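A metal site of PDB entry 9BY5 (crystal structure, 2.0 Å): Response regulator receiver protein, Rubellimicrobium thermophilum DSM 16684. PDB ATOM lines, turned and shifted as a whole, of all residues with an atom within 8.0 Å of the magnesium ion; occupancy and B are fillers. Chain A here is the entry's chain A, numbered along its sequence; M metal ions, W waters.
The guanidinium group of Arg 177 sits at hydrogen-bond distance from the backbone carbonyl oxygen of Asp 153.
NZ of Lys 246 is in salt-bridge range of OD1 of Asp 197, 3.0 Å away.
N of Asp 197 lies within hydrogen-bond range of O of Ile 151 (2.8 Å).
The side-chain carboxylate of Glu 152 sits at hydrogen-bond distance from the backbone NH of Glu 154, at 2.9 Å.
OE1 of Glu 152 lies within salt-bridge range of NZ of Lys 246, 2.8 Å away.
The magnesium ion is bound by water W1, at 2.0 Å.
The magnesium ion is bound by the backbone carbonyl oxygen (O) of Gln 199, 2.0 Å away.
The magnesium ion is bound by OD1 of Asp 153 (2.0 Å).
Water W2 is bound to the magnesium ion, at 2.0 Å.
OD2 of Asp 197 is bound to the magnesium ion, at 2.1 Å.
Water W3 is bound to the magnesium ion (2.2 Å).
OE2 of Glu 152 touches the magnesium ion, at 3.8 Å.
Within 4 Å of the magnesium ion: Glu 152, Asp 153, Asp 197 and Gln 199.
Water W3 bridges the side-chain carboxylate of Asp 153 (2.7 Å) and the side-chain amide oxygen of Gln 199 (3.2 Å).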
ATOM      1  N   ILE A 151      13.144   9.038 -29.311  1.00  0.00           N
ATOM      2  CA  ILE A 151      12.129   8.405 -28.492  1.00  0.00           C
ATOM      3  C   ILE A 151      12.832   7.278 -27.757  1.00  0.00           C
ATOM      4  O   ILE A 151      13.232   6.290 -28.360  1.00  0.00           O
ATOM      5  CB  ILE A 151      10.943   7.902 -29.330  1.00  0.00           C
ATOM      6  CG1 ILE A 151      10.392   9.015 -30.231  1.00  0.00           C
ATOM      7  CG2 ILE A 151       9.863   7.316 -28.400  1.00  0.00           C
ATOM      8  CD1 ILE A 151       9.216   8.610 -31.148  1.00  0.00           C
ATOM      9  N   GLU A 152      13.037   7.476 -26.454  1.00  0.00           N
ATOM     10  CA  GLU A 152      13.850   6.557 -25.660  1.00  0.00           C
ATOM     11  C   GLU A 152      13.587   6.866 -24.203  1.00  0.00           C
ATOM     12  O   GLU A 152      13.678   8.035 -23.801  1.00  0.00           O
ATOM     13  CB  GLU A 152      15.346   6.726 -25.998  1.00  0.00           C
ATOM     14  CG  GLU A 152      16.277   6.092 -24.967  1.00  0.00           C
ATOM     15  CD  GLU A 152      16.183   4.584 -25.015  1.00  0.00           C
ATOM     16  OE1 GLU A 152      16.439   4.009 -26.096  1.00  0.00           O
ATOM     17  OE2 GLU A 152      15.838   3.973 -23.977  1.00  0.00           O
ATOM     18  N   ASP A 153      13.220   5.863 -23.421  1.00  0.00           N
ATOM     19  CA  ASP A 153      12.913   6.099 -22.017  1.00  0.00           C
ATOM     20  C   ASP A 153      14.106   5.933 -21.091  1.00  0.00           C
ATOM     21  O   ASP A 153      14.064   6.435 -19.964  1.00  0.00           O
ATOM     22  CB  ASP A 153      11.802   5.166 -21.547  1.00  0.00           C
ATOM     23  CG  ASP A 153      12.152   3.716 -21.722  1.00  0.00           C
ATOM     24  OD1 ASP A 153      12.679   3.339 -22.798  1.00  0.00           O
ATOM     25  OD2 ASP A 153      11.913   2.948 -20.757  1.00  0.00           O
ATOM     26  N   GLU A 154      15.167   5.239 -21.508  1.00  0.00           N
ATOM     27  CA  GLU A 154      16.373   5.133 -20.688  1.00  0.00           C
ATOM     28  C   GLU A 154      17.220   6.381 -20.856  1.00  0.00           C
ATOM     29  O   GLU A 154      17.793   6.619 -21.937  1.00  0.00           O
ATOM     30  CB  GLU A 154      17.172   3.873 -21.020  1.00  0.00           C
ATOM     31  CG  GLU A 154      16.537   2.615 -20.498  1.00  0.00           C
ATOM     32  CD  GLU A 154      17.397   1.402 -20.739  1.00  0.00           C
ATOM     33  OE1 GLU A 154      18.584   1.432 -20.350  1.00  0.00           O
ATOM     34  OE2 GLU A 154      16.886   0.422 -21.320  1.00  0.00           O
ATOM     35  N   ILE A 157      20.860   6.222 -22.207  1.00  0.00           N
ATOM     36  CA  ILE A 157      20.825   5.976 -23.655  1.00  0.00           C
ATOM     37  C   ILE A 157      20.479   7.251 -24.411  1.00  0.00           C
ATOM     38  O   ILE A 157      21.130   7.597 -25.415  1.00  0.00           O
ATOM     39  CB  ILE A 157      19.823   4.864 -24.002  1.00  0.00           C
ATOM     40  CG1 ILE A 157      19.958   3.669 -23.057  1.00  0.00           C
ATOM     41  CG2 ILE A 157      19.982   4.453 -25.454  1.00  0.00           C
ATOM     42  CD1 ILE A 157      21.052   2.755 -23.429  1.00  0.00           C
ATOM     43  N   ARG A 177       9.926  10.157 -23.750  1.00  0.00           N
ATOM     44  CA  ARG A 177      10.095   8.914 -23.034  1.00  0.00           C
ATOM     45  C   ARG A 177       8.823   8.088 -22.977  1.00  0.00           C
ATOM     46  O   ARG A 177       8.838   6.969 -22.489  1.00  0.00           O
ATOM     47  CB  ARG A 177      10.605   9.191 -21.605  1.00  0.00           C
ATOM     48  CG  ARG A 177      11.928  10.003 -21.578  1.00  0.00           C
ATOM     49  CD  ARG A 177      12.419  10.315 -20.170  1.00  0.00           C
ATOM     50  NE  ARG A 177      12.602   9.087 -19.414  1.00  0.00           N
ATOM     51  CZ  ARG A 177      11.723   8.585 -18.551  1.00  0.00           C
ATOM     52  NH1 ARG A 177      10.700   9.296 -18.112  1.00  0.00           N
ATOM     53  NH2 ARG A 177      11.893   7.341 -18.117  1.00  0.00           N
ATOM     54  N   ALA A 196      13.965   5.753 -32.581  1.00  0.00           N
ATOM     55  CA  ALA A 196      12.867   5.217 -31.781  1.00  0.00           C
ATOM     56  C   ALA A 196      13.243   3.906 -31.103  1.00  0.00           C
ATOM     57  O   ALA A 196      13.632   2.936 -31.762  1.00  0.00           O
ATOM     58  CB  ALA A 196      11.603   5.029 -32.640  1.00  0.00           C
ATOM     59  N   ASP A 197      13.133   3.899 -29.777  1.00  0.00           N
ATOM     60  CA  ASP A 197      13.221   2.691 -28.983  1.00  0.00           C
ATOM     61  C   ASP A 197      11.841   2.052 -29.016  1.00  0.00           C
ATOM     62  O   ASP A 197      10.867   2.704 -29.408  1.00  0.00           O
ATOM     63  CB  ASP A 197      13.675   3.072 -27.570  1.00  0.00           C
ATOM     64  CG  ASP A 197      13.580   1.943 -26.569  1.00  0.00           C
ATOM     65  OD1 ASP A 197      14.108   0.850 -26.869  1.00  0.00           O
ATOM     66  OD2 ASP A 197      13.046   2.173 -25.480  1.00  0.00           O
ATOM     67  N   ILE A 198      11.728   0.784 -28.606  1.00  0.00           N
ATOM     68  CA  ILE A 198      10.427   0.101 -28.624  1.00  0.00           C
ATOM     69  C   ILE A 198       9.648   0.214 -27.315  1.00  0.00           C
ATOM     70  O   ILE A 198       8.523   0.716 -27.282  1.00  0.00           O
ATOM     71  CB  ILE A 198      10.585  -1.385 -28.969  1.00  0.00           C
ATOM     72  CG1 ILE A 198      11.489  -1.559 -30.167  1.00  0.00           C
ATOM     73  CG2 ILE A 198       9.230  -1.999 -29.223  1.00  0.00           C
ATOM     74  CD1 ILE A 198      10.779  -1.551 -31.436  1.00  0.00           C
ATOM     75  N   GLN A 199      10.204  -0.321 -26.229  1.00  0.00           N
ATOM     76  CA  GLN A 199       9.523  -0.290 -24.938  1.00  0.00           C
ATOM     77  C   GLN A 199       9.843   1.023 -24.231  1.00  0.00           C
ATOM     78  O   GLN A 199      11.011   1.305 -23.956  1.00  0.00           O
ATOM     79  CB  GLN A 199       9.940  -1.477 -24.063  1.00  0.00           C
ATOM     80  CG  GLN A 199       9.000  -1.780 -22.891  1.00  0.00           C
ATOM     81  CD  GLN A 199       9.547  -1.330 -21.527  1.00  0.00           C
ATOM     82  OE1 GLN A 199      10.581  -1.823 -21.063  1.00  0.00           O
ATOM     83  NE2 GLN A 199       8.848  -0.398 -20.879  1.00  0.00           N
ATOM     84  N   LEU A 200       8.805   1.805 -23.931  1.00  0.00           N
ATOM     85  CA  LEU A 200       8.954   3.137 -23.369  1.00  0.00           C
ATOM     86  C   LEU A 200       8.621   3.108 -21.876  1.00  0.00           C
ATOM     87  O   LEU A 200       8.308   2.060 -21.309  1.00  0.00           O
ATOM     88  CB  LEU A 200       8.082   4.123 -24.139  1.00  0.00           C
ATOM     89  CG  LEU A 200       8.491   4.202 -25.618  1.00  0.00           C
ATOM     90  CD1 LEU A 200       7.678   5.269 -26.359  1.00  0.00           C
ATOM     91  CD2 LEU A 200       9.992   4.478 -25.735  1.00  0.00           C
ATOM     92  N   ALA A 201       8.663   4.286 -21.239  1.00  0.00           N
ATOM     93  CA  ALA A 201       8.671   4.338 -19.771  1.00  0.00           C
ATOM     94  C   ALA A 201       7.369   3.840 -19.178  1.00  0.00           C
ATOM     95  O   ALA A 201       7.375   3.100 -18.186  1.00  0.00           O
ATOM     96  CB  ALA A 201       8.948   5.765 -19.297  1.00  0.00           C
ATOM     97  N   SER A 204       4.119   1.786 -22.845  1.00  0.00           N
ATOM     98  CA  SER A 204       3.681   1.978 -24.227  1.00  0.00           C
ATOM     99  C   SER A 204       4.825   1.698 -25.222  1.00  0.00           C
ATOM    100  O   SER A 204       5.996   1.565 -24.848  1.00  0.00           O
ATOM    101  CB  SER A 204       3.118   3.380 -24.422  1.00  0.00           C
ATOM    102  OG  SER A 204       4.150   4.358 -24.298  1.00  0.00           O
ATOM    103  N   GLY A 206       7.135   2.337 -28.691  1.00  0.00           N
ATOM    104  CA  GLY A 206       7.600   3.269 -29.701  1.00  0.00           C
ATOM    105  C   GLY A 206       7.029   2.977 -31.079  1.00  0.00           C
ATOM    106  O   GLY A 206       6.938   3.873 -31.915  1.00  0.00           O
ATOM    107  N   ILE A 225      15.871   1.406 -32.751  1.00  0.00           N
ATOM    108  CA  ILE A 225      17.042   0.922 -32.015  1.00  0.00           C
ATOM    109  C   ILE A 225      16.525  -0.029 -30.950  1.00  0.00           C
ATOM    110  O   ILE A 225      15.803   0.393 -30.038  1.00  0.00           O
ATOM    111  CB  ILE A 225      17.829   2.075 -31.370  1.00  0.00           C
ATOM    112  CG1 ILE A 225      18.202   3.097 -32.443  1.00  0.00           C
ATOM    113  CG2 ILE A 225      19.067   1.544 -30.699  1.00  0.00           C
ATOM    114  CD1 ILE A 225      18.467   4.521 -31.924  1.00  0.00           C
ATOM    115  N   LYS A 246      20.662  -3.069 -30.014  1.00  0.00           N
ATOM    116  CA  LYS A 246      21.112  -2.630 -28.676  1.00  0.00           C
ATOM    117  C   LYS A 246      21.784  -3.865 -28.064  1.00  0.00           C
ATOM    118  O   LYS A 246      21.103  -4.899 -27.964  1.00  0.00           O
ATOM    119  CB  LYS A 246      19.968  -2.162 -27.783  1.00  0.00           C
ATOM    120  CG  LYS A 246      19.244  -0.943 -28.285  1.00  0.00           C
ATOM    121  CD  LYS A 246      18.088  -0.518 -27.396  1.00  0.00           C
ATOM    122  CE  LYS A 246      17.963   0.961 -27.278  1.00  0.00           C
ATOM    123  NZ  LYS A 246      17.030   1.300 -26.201  1.00  0.00           N
HETATM  124 MG    MG M   1      12.978   1.475 -23.529  1.00  0.00          MG
HETATM  125  O   HOH W   1      13.362  -0.213 -24.442  1.00  0.00           O
HETATM  126  O   HOH W   2      15.011   1.609 -23.581  1.00  0.00           O
HETATM  127  O   HOH W   3      12.669   0.523 -21.608  1.00  0.00           O
